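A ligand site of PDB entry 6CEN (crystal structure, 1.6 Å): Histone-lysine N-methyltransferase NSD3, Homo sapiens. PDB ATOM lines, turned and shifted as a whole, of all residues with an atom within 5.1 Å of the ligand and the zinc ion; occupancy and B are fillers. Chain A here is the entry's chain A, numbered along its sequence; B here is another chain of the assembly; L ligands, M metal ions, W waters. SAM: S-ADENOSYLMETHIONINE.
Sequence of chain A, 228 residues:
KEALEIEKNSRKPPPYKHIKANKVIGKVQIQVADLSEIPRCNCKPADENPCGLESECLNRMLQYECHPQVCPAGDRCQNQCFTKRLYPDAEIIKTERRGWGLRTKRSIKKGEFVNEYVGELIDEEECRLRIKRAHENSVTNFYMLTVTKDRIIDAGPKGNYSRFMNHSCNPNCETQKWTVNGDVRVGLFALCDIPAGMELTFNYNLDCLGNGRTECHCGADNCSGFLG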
ATOM      1  N   ARG A  97       9.686  -0.922  15.665  1.00  0.00           N
ATOM      2  CA  ARG A  97       9.008  -1.989  14.934  1.00  0.00           C
ATOM      3  C   ARG A  97       8.721  -3.265  15.720  1.00  0.00           C
ATOM      4  O   ARG A  97       8.128  -4.197  15.180  1.00  0.00           O
ATOM      5  CB  ARG A  97       9.858  -2.334  13.723  1.00  0.00           C
ATOM      6  CG  ARG A  97       9.848  -1.219  12.699  1.00  0.00           C
ATOM      7  CD  ARG A  97       8.696  -1.399  11.712  1.00  0.00           C
ATOM      8  NE  ARG A  97       9.221  -1.925  10.462  1.00  0.00           N
ATOM      9  CZ  ARG A  97       8.515  -2.463   9.476  1.00  0.00           C
ATOM     10  NH1 ARG A  97       9.165  -2.855   8.389  1.00  0.00           N
ATOM     11  NH2 ARG A  97       7.199  -2.631   9.559  1.00  0.00           N
ATOM     12  N   ARG A  98       9.125  -3.285  16.984  1.00  0.00           N
ATOM     13  CA  ARG A  98       8.998  -4.459  17.842  1.00  0.00           C
ATOM     14  C   ARG A  98       8.248  -4.089  19.135  1.00  0.00           C
ATOM     15  O   ARG A  98       8.348  -4.766  20.138  1.00  0.00           O
ATOM     16  CB  ARG A  98      10.362  -5.091  18.124  1.00  0.00           C
ATOM     17  CG  ARG A  98      11.068  -5.576  16.853  1.00  0.00           C
ATOM     18  CD  ARG A  98      12.473  -6.096  17.090  1.00  0.00           C
ATOM     19  NE  ARG A  98      13.332  -4.998  17.495  1.00  0.00           N
ATOM     20  CZ  ARG A  98      13.773  -4.748  18.720  1.00  0.00           C
ATOM     21  NH1 ARG A  98      13.621  -5.643  19.690  1.00  0.00           N
ATOM     22  NH2 ARG A  98      14.446  -3.628  18.975  1.00  0.00           N
ATOM     23  N   GLY A  99       7.462  -3.012  19.077  1.00  0.00           N
ATOM     24  CA  GLY A  99       6.638  -2.616  20.209  1.00  0.00           C
ATOM     25  C   GLY A  99       7.492  -2.176  21.365  1.00  0.00           C
ATOM     26  O   GLY A  99       8.557  -1.575  21.183  1.00  0.00           O
ATOM     27  N   TRP A 100       7.040  -2.506  22.568  1.00  0.00           N
ATOM     28  CA  TRP A 100       7.799  -2.262  23.776  1.00  0.00           C
ATOM     29  C   TRP A 100       8.821  -3.395  23.971  1.00  0.00           C
ATOM     30  O   TRP A 100       8.549  -4.535  23.588  1.00  0.00           O
ATOM     31  CB  TRP A 100       6.863  -2.172  24.970  1.00  0.00           C
ATOM     32  CG  TRP A 100       5.929  -1.026  24.807  1.00  0.00           C
ATOM     33  CD1 TRP A 100       4.682  -1.056  24.270  1.00  0.00           C
ATOM     34  CD2 TRP A 100       6.196   0.329  25.137  1.00  0.00           C
ATOM     35  NE1 TRP A 100       4.143   0.192  24.255  1.00  0.00           N
ATOM     36  CE2 TRP A 100       5.050   1.073  24.787  1.00  0.00           C
ATOM     37  CE3 TRP A 100       7.284   0.977  25.702  1.00  0.00           C
ATOM     38  CZ2 TRP A 100       4.956   2.434  24.990  1.00  0.00           C
ATOM     39  CZ3 TRP A 100       7.195   2.378  25.904  1.00  0.00           C
ATOM     40  CH2 TRP A 100       6.036   3.076  25.553  1.00  0.00           C
ATOM     41  N   GLY A 101      10.002  -3.044  24.441  1.00  0.00           N
ATOM     42  CA  GLY A 101      11.057  -4.007  24.737  1.00  0.00           C
ATOM     43  C   GLY A 101      11.582  -3.833  26.140  1.00  0.00           C
ATOM     44  O   GLY A 101      11.024  -3.056  26.924  1.00  0.00           O
ATOM     45  N   TYR A 117      10.354 -16.143  33.813  1.00  0.00           N
ATOM     46  CA  TYR A 117       9.174 -15.937  32.950  1.00  0.00           C
ATOM     47  C   TYR A 117       7.943 -16.329  33.739  1.00  0.00           C
ATOM     48  O   TYR A 117       7.694 -17.509  33.941  1.00  0.00           O
ATOM     49  CB  TYR A 117       9.281 -16.728  31.625  1.00  0.00           C
ATOM     50  CG  TYR A 117       8.362 -16.231  30.560  1.00  0.00           C
ATOM     51  CD1 TYR A 117       8.757 -15.203  29.705  1.00  0.00           C
ATOM     52  CD2 TYR A 117       7.090 -16.775  30.384  1.00  0.00           C
ATOM     53  CE1 TYR A 117       7.912 -14.692  28.742  1.00  0.00           C
ATOM     54  CE2 TYR A 117       6.223 -16.296  29.406  1.00  0.00           C
ATOM     55  CZ  TYR A 117       6.634 -15.277  28.567  1.00  0.00           C
ATOM     56  OH  TYR A 117       5.805 -14.746  27.625  1.00  0.00           O
ATOM     57  N   THR A 140      -1.857  -8.825  17.955  1.00  0.00           N
ATOM     58  CA  THR A 140      -0.611  -9.287  17.334  1.00  0.00           C
ATOM     59  C   THR A 140       0.547  -9.562  18.311  1.00  0.00           C
ATOM     60  O   THR A 140       1.627  -9.981  17.883  1.00  0.00           O
ATOM     61  CB  THR A 140      -0.165  -8.291  16.272  1.00  0.00           C
ATOM     62  OG1 THR A 140       0.120  -7.031  16.891  1.00  0.00           O
ATOM     63  CG2 THR A 140      -1.307  -8.110  15.218  1.00  0.00           C
ATOM     64  N   ASN A 141       0.293  -9.369  19.597  1.00  0.00           N
ATOM     65  CA  ASN A 141       1.252  -9.657  20.647  1.00  0.00           C
ATOM     66  C   ASN A 141       0.818 -10.903  21.386  1.00  0.00           C
ATOM     67  O   ASN A 141      -0.314 -10.983  21.842  1.00  0.00           O
ATOM     68  CB  ASN A 141       1.322  -8.465  21.588  1.00  0.00           C
ATOM     69  CG  ASN A 141       2.070  -7.308  20.969  1.00  0.00           C
ATOM     70  OD1 ASN A 141       3.285  -7.280  20.969  1.00  0.00           O
ATOM     71  ND2 ASN A 141       1.346  -6.358  20.420  1.00  0.00           N
ATOM     72  N   PHE A 142       1.731 -11.866  21.469  1.00  0.00           N
ATOM     73  CA  PHE A 142       1.491 -13.134  22.151  1.00  0.00           C
ATOM     74  C   PHE A 142       2.568 -13.372  23.180  1.00  0.00           C
ATOM     75  O   PHE A 142       3.720 -13.042  22.929  1.00  0.00           O
ATOM     76  CB  PHE A 142       1.417 -14.241  21.131  1.00  0.00           C
ATOM     77  CG  PHE A 142       0.229 -14.109  20.240  1.00  0.00           C
ATOM     78  CD1 PHE A 142       0.297 -13.341  19.094  1.00  0.00           C
ATOM     79  CD2 PHE A 142      -0.990 -14.675  20.598  1.00  0.00           C
ATOM     80  CE1 PHE A 142      -0.814 -13.182  18.267  1.00  0.00           C
ATOM     81  CE2 PHE A 142      -2.107 -14.514  19.783  1.00  0.00           C
ATOM     82  CZ  PHE A 142      -2.018 -13.764  18.625  1.00  0.00           C
ATOM     83  N   TYR A 143       2.153 -13.872  24.353  1.00  0.00           N
ATOM     84  CA  TYR A 143       3.027 -14.005  25.522  1.00  0.00           C
ATOM     85  C   TYR A 143       2.987 -15.433  26.091  1.00  0.00           C
ATOM     86  O   TYR A 143       3.323 -15.635  27.262  1.00  0.00           O
ATOM     87  CB  TYR A 143       2.608 -13.020  26.624  1.00  0.00           C
ATOM     88  CG  TYR A 143       2.518 -11.578  26.181  1.00  0.00           C
ATOM     89  CD1 TYR A 143       1.450 -11.133  25.450  1.00  0.00           C
ATOM     90  CD2 TYR A 143       3.519 -10.648  26.534  1.00  0.00           C
ATOM     91  CE1 TYR A 143       1.374  -9.810  25.032  1.00  0.00           C
ATOM     92  CE2 TYR A 143       3.450  -9.319  26.118  1.00  0.00           C
ATOM     93  CZ  TYR A 143       2.394  -8.893  25.363  1.00  0.00           C
ATOM     94  OH  TYR A 143       2.310  -7.559  24.940  1.00  0.00           O
ATOM     95  N   ARG A 163       7.960 -10.221  30.285  1.00  0.00           N
ATOM     96  CA  ARG A 163       6.939 -10.227  29.241  1.00  0.00           C
ATOM     97  C   ARG A 163       7.287  -9.240  28.126  1.00  0.00           C
ATOM     98  O   ARG A 163       6.732  -9.307  27.028  1.00  0.00           O
ATOM     99  CB  ARG A 163       5.539  -9.890  29.787  1.00  0.00           C
ATOM    100  CG  ARG A 163       5.364  -8.424  30.138  1.00  0.00           C
ATOM    101  CD  ARG A 163       4.099  -8.225  30.914  1.00  0.00           C
ATOM    102  NE  ARG A 163       2.918  -8.466  30.114  1.00  0.00           N
ATOM    103  CZ  ARG A 163       2.375  -7.565  29.309  1.00  0.00           C
ATOM    104  NH1 ARG A 163       2.995  -6.417  29.046  1.00  0.00           N
ATOM    105  NH2 ARG A 163       1.255  -7.850  28.673  1.00  0.00           N
ATOM    106  N   PHE A 164       8.172  -8.295  28.455  1.00  0.00           N
ATOM    107  CA  PHE A 164       8.626  -7.300  27.483  1.00  0.00           C
ATOM    108  C   PHE A 164       9.808  -7.694  26.654  1.00  0.00           C
ATOM    109  O   PHE A 164      10.163  -6.971  25.738  1.00  0.00           O
ATOM    110  CB  PHE A 164       8.902  -5.957  28.184  1.00  0.00           C
ATOM    111  CG  PHE A 164       7.659  -5.280  28.693  1.00  0.00           C
ATOM    112  CD1 PHE A 164       6.770  -4.688  27.804  1.00  0.00           C
ATOM    113  CD2 PHE A 164       7.324  -5.288  30.039  1.00  0.00           C
ATOM    114  CE1 PHE A 164       5.634  -4.055  28.242  1.00  0.00           C
ATOM    115  CE2 PHE A 164       6.183  -4.666  30.483  1.00  0.00           C
ATOM    116  CZ  PHE A 164       5.327  -4.062  29.585  1.00  0.00           C
ATOM    117  N   MET A 165      10.440  -8.829  26.928  1.00  0.00           N
ATOM    118  CA  MET A 165      11.636  -9.214  26.183  1.00  0.00           C
ATOM    119  C   MET A 165      11.271  -9.682  24.794  1.00  0.00           C
ATOM    120  O   MET A 165      10.457 -10.584  24.618  1.00  0.00           O
ATOM    121  CB  MET A 165      12.393 -10.303  26.939  1.00  0.00           C
ATOM    122  CG  MET A 165      13.131  -9.683  28.127  1.00  0.00           C
ATOM    123  SD  MET A 165      13.936 -10.877  29.187  1.00  0.00           S
ATOM    124  CE  MET A 165      15.104 -11.608  28.047  1.00  0.00           C
ATOM    125  N   ASN A 166      11.840  -9.010  23.801  1.00  0.00           N
ATOM    126  CA  ASN A 166      11.587  -9.374  22.422  1.00  0.00           C
ATOM    127  C   ASN A 166      12.364 -10.575  21.917  1.00  0.00           C
ATOM    128  O   ASN A 166      13.393 -10.987  22.488  1.00  0.00           O
ATOM    129  CB  ASN A 166      11.780  -8.154  21.535  1.00  0.00           C
ATOM    130  CG  ASN A 166      10.646  -7.176  21.670  1.00  0.00           C
ATOM    131  OD1 ASN A 166       9.479  -7.586  21.672  1.00  0.00           O
ATOM    132  ND2 ASN A 166      10.947  -5.893  21.749  1.00  0.00           N
ATOM    133  N   HIS A 167      11.858 -11.130  20.806  1.00  0.00           N
ATOM    134  CA  HIS A 167      12.539 -12.213  20.091  1.00  0.00           C
ATOM    135  C   HIS A 167      13.734 -11.699  19.328  1.00  0.00           C
ATOM    136  O   HIS A 167      13.636 -10.683  18.662  1.00  0.00           O
ATOM    137  CB  HIS A 167      11.600 -12.886  19.081  1.00  0.00           C
ATOM    138  CG  HIS A 167      12.315 -13.779  18.122  1.00  0.00           C
ATOM    139  ND1 HIS A 167      12.700 -15.047  18.443  1.00  0.00           N
ATOM    140  CD2 HIS A 167      12.817 -13.537  16.887  1.00  0.00           C
ATOM    141  CE1 HIS A 167      13.377 -15.581  17.435  1.00  0.00           C
ATOM    142  NE2 HIS A 167      13.467 -14.669  16.482  1.00  0.00           N
ATOM    143  N   SER A 168      14.845 -12.428  19.403  1.00  0.00           N
ATOM    144  CA  SER A 168      15.925 -12.236  18.452  1.00  0.00           C
ATOM    145  C   SER A 168      16.400 -13.539  17.881  1.00  0.00           C
ATOM    146  O   SER A 168      16.472 -14.553  18.574  1.00  0.00           O
ATOM    147  CB  SER A 168      17.112 -11.504  19.110  1.00  0.00           C
ATOM    148  OG  SER A 168      18.185 -11.322  18.165  1.00  0.00           O
ATOM    149  N   CYS A 169      16.762 -13.511  16.600  1.00  0.00           N
ATOM    150  CA  CYS A 169      17.442 -14.600  15.940  1.00  0.00           C
ATOM    151  C   CYS A 169      18.904 -14.777  16.360  1.00  0.00           C
ATOM    152  O   CYS A 169      19.491 -15.852  16.131  1.00  0.00           O
ATOM    153  CB  CYS A 169      17.340 -14.386  14.415  1.00  0.00           C
ATOM    154  SG  CYS A 169      15.607 -14.340  13.804  1.00  0.00           S
ATOM    155  N   TYR A 204      12.448 -17.101  20.827  1.00  0.00           N
ATOM    156  CA  TYR A 204      11.126 -17.638  21.167  1.00  0.00           C
ATOM    157  C   TYR A 204      10.920 -19.096  20.773  1.00  0.00           C
ATOM    158  O   TYR A 204      10.105 -19.763  21.372  1.00  0.00           O
ATOM    159  CB  TYR A 204      10.033 -16.808  20.514  1.00  0.00           C
ATOM    160  CG  TYR A 204       9.776 -15.425  21.093  1.00  0.00           C
ATOM    161  CD1 TYR A 204      10.606 -14.839  22.045  1.00  0.00           C
ATOM    162  CD2 TYR A 204       8.734 -14.652  20.586  1.00  0.00           C
ATOM    163  CE1 TYR A 204      10.358 -13.552  22.535  1.00  0.00           C
ATOM    164  CE2 TYR A 204       8.490 -13.370  21.039  1.00  0.00           C
ATOM    165  CZ  TYR A 204       9.288 -12.822  22.019  1.00  0.00           C
ATOM    166  OH  TYR A 204       8.985 -11.544  22.453  1.00  0.00           O
ATOM    167  N   GLU A 215       6.431 -11.175  10.623  1.00  0.00           N
ATOM    168  CA  GLU A 215       7.732 -10.676  10.207  1.00  0.00           C
ATOM    169  C   GLU A 215       8.626 -10.384  11.425  1.00  0.00           C
ATOM    170  O   GLU A 215       8.161  -9.853  12.429  1.00  0.00           O
ATOM    171  CB  GLU A 215       7.517  -9.402   9.387  1.00  0.00           C
ATOM    172  CG  GLU A 215       8.747  -8.714   8.820  1.00  0.00           C
ATOM    173  CD  GLU A 215       8.375  -7.583   7.870  1.00  0.00           C
ATOM    174  OE1 GLU A 215       7.171  -7.296   7.722  1.00  0.00           O
ATOM    175  OE2 GLU A 215       9.283  -6.971   7.264  1.00  0.00           O
ATOM    176  N   CYS A 216       9.913 -10.719  11.319  1.00  0.00           N
ATOM    177  CA  CYS A 216      10.877 -10.440  12.383  1.00  0.00           C
ATOM    178  C   CYS A 216      11.686  -9.192  12.050  1.00  0.00           C
ATOM    179  O   CYS A 216      12.204  -9.082  10.935  1.00  0.00           O
ATOM    180  CB  CYS A 216      11.819 -11.625  12.616  1.00  0.00           C
ATOM    181  SG  CYS A 216      12.946 -11.385  14.008  1.00  0.00           S
ATOM    182  N   HIS A 217      11.811  -8.292  13.018  1.00  0.00           N
ATOM    183  CA  HIS A 217      12.643  -7.088  12.910  1.00  0.00           C
ATOM    184  C   HIS A 217      13.824  -7.063  13.854  1.00  0.00           C
ATOM    185  O   HIS A 217      14.295  -5.992  14.279  1.00  0.00           O
ATOM    186  CB  HIS A 217      11.777  -5.827  13.033  1.00  0.00           C
ATOM    187  CG  HIS A 217      10.705  -5.751  12.004  1.00  0.00           C
ATOM    188  ND1 HIS A 217      10.977  -5.482  10.685  1.00  0.00           N
ATOM    189  CD2 HIS A 217       9.367  -5.910  12.085  1.00  0.00           C
ATOM    190  CE1 HIS A 217       9.850  -5.500   9.991  1.00  0.00           C
ATOM    191  NE2 HIS A 217       8.866  -5.749  10.819  1.00  0.00           N
ATOM    192  N   CYS A 218      14.357  -8.254  14.189  1.00  0.00           N
ATOM    193  CA  CYS A 218      15.418  -8.304  15.186  1.00  0.00           C
ATOM    194  C   CYS A 218      16.718  -7.664  14.734  1.00  0.00           C
ATOM    195  O   CYS A 218      17.518  -7.239  15.554  1.00  0.00           O
ATOM    196  CB  CYS A 218      15.676  -9.739  15.682  1.00  0.00           C
ATOM    197  SG  CYS A 218      16.615 -10.810  14.553  1.00  0.00           S
ATOM    198  N   GLY A 219      16.935  -7.622  13.433  1.00  0.00           N
ATOM    199  CA  GLY A 219      18.113  -6.967  12.899  1.00  0.00           C
ATOM    200  C   GLY A 219      19.376  -7.847  12.815  1.00  0.00           C
ATOM    201  O   GLY A 219      20.427  -7.387  12.304  1.00  0.00           O
ATOM    202  N   CYS A 223      19.012 -13.339  10.765  1.00  0.00           N
ATOM    203  CA  CYS A 223      17.555 -13.275  10.856  1.00  0.00           C
ATOM    204  C   CYS A 223      16.900 -14.081   9.739  1.00  0.00           C
ATOM    205  O   CYS A 223      17.256 -13.895   8.582  1.00  0.00           O
ATOM    206  CB  CYS A 223      17.065 -11.854  10.748  1.00  0.00           C
ATOM    207  SG  CYS A 223      15.290 -11.742  11.087  1.00  0.00           S
ATOM    208  N   SER A 224      15.958 -14.945  10.071  1.00  0.00           N
ATOM    209  CA  SER A 224      15.246 -15.757   9.083  1.00  0.00           C
ATOM    210  C   SER A 224      14.267 -14.906   8.302  1.00  0.00           C
ATOM    211  O   SER A 224      13.830 -15.316   7.217  1.00  0.00           O
ATOM    212  CB  SER A 224      14.479 -16.887   9.730  1.00  0.00           C
ATOM    213  OG  SER A 224      13.377 -16.384  10.460  1.00  0.00           O
ATOM    214  N   GLY A 225      13.878 -13.776   8.905  1.00  0.00           N
ATOM    215  CA  GLY A 225      12.846 -12.883   8.384  1.00  0.00           C
ATOM    216  C   GLY A 225      11.523 -13.106   9.093  1.00  0.00           C
ATOM    217  O   GLY A 225      10.591 -12.316   8.916  1.00  0.00           O
ATOM    218  N   PHE A 226      11.423 -14.150   9.905  1.00  0.00           N
ATOM    219  CA  PHE A 226      10.178 -14.505  10.498  1.00  0.00           C
ATOM    220  C   PHE A 226      10.331 -14.814  11.929  1.00  0.00           C
ATOM    221  O   PHE A 226      11.341 -15.365  12.402  1.00  0.00           O
ATOM    222  CB  PHE A 226       9.507 -15.690   9.804  1.00  0.00           C
ATOM    223  CG  PHE A 226       9.385 -15.498   8.350  1.00  0.00           C
ATOM    224  CD1 PHE A 226       8.391 -14.671   7.844  1.00  0.00           C
ATOM    225  CD2 PHE A 226      10.264 -16.130   7.482  1.00  0.00           C
ATOM    226  CE1 PHE A 226       8.278 -14.481   6.480  1.00  0.00           C
ATOM    227  CE2 PHE A 226      10.150 -15.940   6.118  1.00  0.00           C
ATOM    228  CZ  PHE A 226       9.143 -15.113   5.614  1.00  0.00           C
ATOM    229  N   LEU A 227       9.272 -14.453  12.622  1.00  0.00           N
ATOM    230  CA  LEU A 227       9.310 -14.374  14.029  1.00  0.00           C
ATOM    231  C   LEU A 227       9.342 -15.767  14.620  1.00  0.00           C
ATOM    232  O   LEU A 227       8.674 -16.693  14.115  1.00  0.00           O
ATOM    233  CB  LEU A 227       8.110 -13.564  14.515  1.00  0.00           C
ATOM    234  CG  LEU A 227       8.122 -13.197  15.971  1.00  0.00           C
ATOM    235  CD1 LEU A 227       9.256 -12.241  16.241  1.00  0.00           C
ATOM    236  CD2 LEU A 227       6.774 -12.587  16.329  1.00  0.00           C
ATOM    237  N   NLE B   4       5.680 -19.963  22.492  1.00  0.00           N
ATOM    238  CA  NLE B   4       7.100 -20.065  22.660  1.00  0.00           C
ATOM    239  C   NLE B   4       7.442 -21.407  23.232  1.00  0.00           C
ATOM    240  O   NLE B   4       6.659 -22.011  23.966  1.00  0.00           O
ATOM    241  CB  NLE B   4       7.642 -18.976  23.592  1.00  0.00           C
ATOM    242  CG  NLE B   4       7.254 -17.527  23.223  1.00  0.00           C
ATOM    243  CD  NLE B   4       7.603 -16.589  24.392  1.00  0.00           C
ATOM    244  CE  NLE B   4       7.184 -15.165  24.127  1.00  0.00           C
HETATM  245  N   SAM L   1       6.992  -6.172  22.069  1.00  0.00           N
HETATM  246  CA  SAM L   1       6.032  -6.749  23.023  1.00  0.00           C
HETATM  247  C   SAM L   1       5.112  -5.661  23.550  1.00  0.00           C
HETATM  248  O   SAM L   1       4.350  -5.883  24.539  1.00  0.00           O
HETATM  249  OXT SAM L   1       5.145  -4.556  22.952  1.00  0.00           O
HETATM  250  CB  SAM L   1       6.784  -7.498  24.128  1.00  0.00           C
HETATM  251  CG  SAM L   1       7.115  -8.952  23.777  1.00  0.00           C
HETATM  252  SD  SAM L   1       5.785  -9.971  23.586  1.00  0.00           S
HETATM  253  CE  SAM L   1       6.093 -11.283  24.546  1.00  0.00           C
HETATM  254  C5' SAM L   1       5.896 -10.661  22.052  1.00  0.00           C
HETATM  255  C4' SAM L   1       5.354  -9.890  20.854  1.00  0.00           C
HETATM  256  O4' SAM L   1       6.217  -8.822  20.506  1.00  0.00           O
HETATM  257  C3' SAM L   1       5.264 -10.756  19.602  1.00  0.00           C
HETATM  258  O3' SAM L   1       4.024 -11.470  19.558  1.00  0.00           O
HETATM  259  C2' SAM L   1       5.428  -9.741  18.502  1.00  0.00           C
HETATM  260  O2' SAM L   1       4.176  -9.098  18.269  1.00  0.00           O
HETATM  261  C1' SAM L   1       6.408  -8.734  19.095  1.00  0.00           C
HETATM  262  N9  SAM L   1       7.808  -9.070  18.768  1.00  0.00           N
HETATM  263  C8  SAM L   1       8.718  -9.628  19.593  1.00  0.00           C
HETATM  264  N7  SAM L   1       9.917  -9.815  19.004  1.00  0.00           N
HETATM  265  C5  SAM L   1       9.755  -9.295  17.760  1.00  0.00           C
HETATM  266  C6  SAM L   1      10.624  -9.210  16.590  1.00  0.00           C
HETATM  267  N6  SAM L   1      11.870  -9.617  16.690  1.00  0.00           N
HETATM  268  N1  SAM L   1      10.098  -8.679  15.475  1.00  0.00           N
HETATM  269  C2  SAM L   1       8.818  -8.272  15.391  1.00  0.00           C
HETATM  270  N3  SAM L   1       7.948  -8.325  16.417  1.00  0.00           N
HETATM  271  C4  SAM L   1       8.388  -8.865  17.595  1.00  0.00           C
HETATM  272 ZN    ZN M   1      15.065 -12.110  13.358  1.00  0.00          ZN
HETATM  273  O   HOH W   1       2.958  -6.656  17.307  1.00  0.00           O
HETATM  274  O   HOH W   2       5.087  -5.680  19.795  1.00  0.00           O
HETATM  275  O   HOH W   3       2.720  -3.897  25.372  1.00  0.00           O
HETATM  276  O   HOH W   4       3.185  -3.548  21.223  1.00  0.00           O
HETATM  277  O   HOH W   5       5.573  -7.315  15.302  1.00  0.00           O
HETATM  278  O   HOH W   6       4.728 -13.927  18.710  1.00  0.00           O
HETATM  279  O   HOH W   7       8.766 -12.244  26.379  1.00  0.00           O
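N6 of the ligand sits close to SG of Cys 216, 3.4 Å away.
A nitrogen (N) of the ligand lies within hydrogen-bond range of the side-chain amide oxygen (OD1) of Asn 166 (2.9 Å).
The side-chain hydroxyl of Tyr 143 sits at hydrogen-bond distance from an oxygen (O) of the ligand (2.7 Å).
A nitrogen (N) of the ligand sits at hydrogen-bond distance from the backbone carbonyl oxygen of Arg 98, at 2.7 Å.
The backbone carbonyl oxygen (O) of Thr 140 lies within hydrogen-bond range of an oxygen (O2') of the ligand.
The backbone carbonyl oxygen (O) of Trp 100 is in hydrogen-bond range of a nitrogen (N) of the ligand.
N of Trp 100 is in hydrogen-bond range of OXT of the ligand, at 2.8 Å.
O4' of the ligand sits close to OD1 of Asn 141 (3.3 Å).
The backbone NH (N) of His 167 lies within hydrogen-bond range of a nitrogen (N7) of the ligand (3.0 Å).
An oxygen (O3') of the ligand is in hydrogen-bond range of the backbone NH (N) of Phe 142 (3.0 Å).
The backbone NH (N) of His 217 lies within hydrogen-bond range of a nitrogen (N1) of the ligand, at 3.0 Å.
N6 of the ligand is in hydrogen-bond range of O of His 167 (2.9 Å).
O of Arg 98 lies within hydrogen-bond range of ND2 of Asn 166, 3.3 Å away.
SG of Cys 223 sits close to N of Gly 225, at 3.3 Å.
N of Cys 169 is in hydrogen-bond range of NE2 of His 167 (3.5 Å).
The side-chain hydroxyl of Tyr 204 sits at hydrogen-bond distance from the backbone carbonyl oxygen of Met 165 (2.8 Å).
The backbone carbonyl oxygen (O) of Tyr 143 lies within hydrogen-bond range of the side-chain hydroxyl (OH) of Tyr 117 (2.7 Å).
SG of Cys 169 lies close to N of Ser 224 (3.8 Å).
ND1 of His 167 sits at hydrogen-bond distance from N of Tyr 204.
The backbone NH of Cys 216 is in hydrogen-bond range of the backbone carbonyl oxygen of Gly 225 (3.0 Å).
SD of the ligand sits close to O of Arg 163 (3.6 Å).
OH of Tyr 204 sits close to SD of the ligand, at 3.7 Å.
Residues that only touch the ligand: Leu 227, Glu 215, Gly 99, Phe 164 and Met 165.
Hydrophobic or aromatic side chains that line the ligand: Trp 100, Tyr 143, His 167, Tyr 204 and Leu 227.
Four residues have an atom within 4 Å of the zinc ion: Cys 169, Cys 216, Cys 218 and Cys 223.
The zinc ion is bound by the side-chain sulfur (SG) of Cys 223, the side-chain sulfur (SG) of Cys 216, the side-chain sulfur (SG) of Cys 169 and the side-chain sulfur (SG) of Cys 218.
Water W4 lies within hydrogen-bond range of an oxygen (OXT) of the ligand and the side-chain amide nitrogen of Asn 141.
Water W1 lies within hydrogen-bond range of OG1 of Thr 140 (2.9 Å) and O2' of the ligand (2.9 Å).
Water W2 lies within hydrogen-bond range of OD1 of Asn 141, N of the ligand and O of Arg 98.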
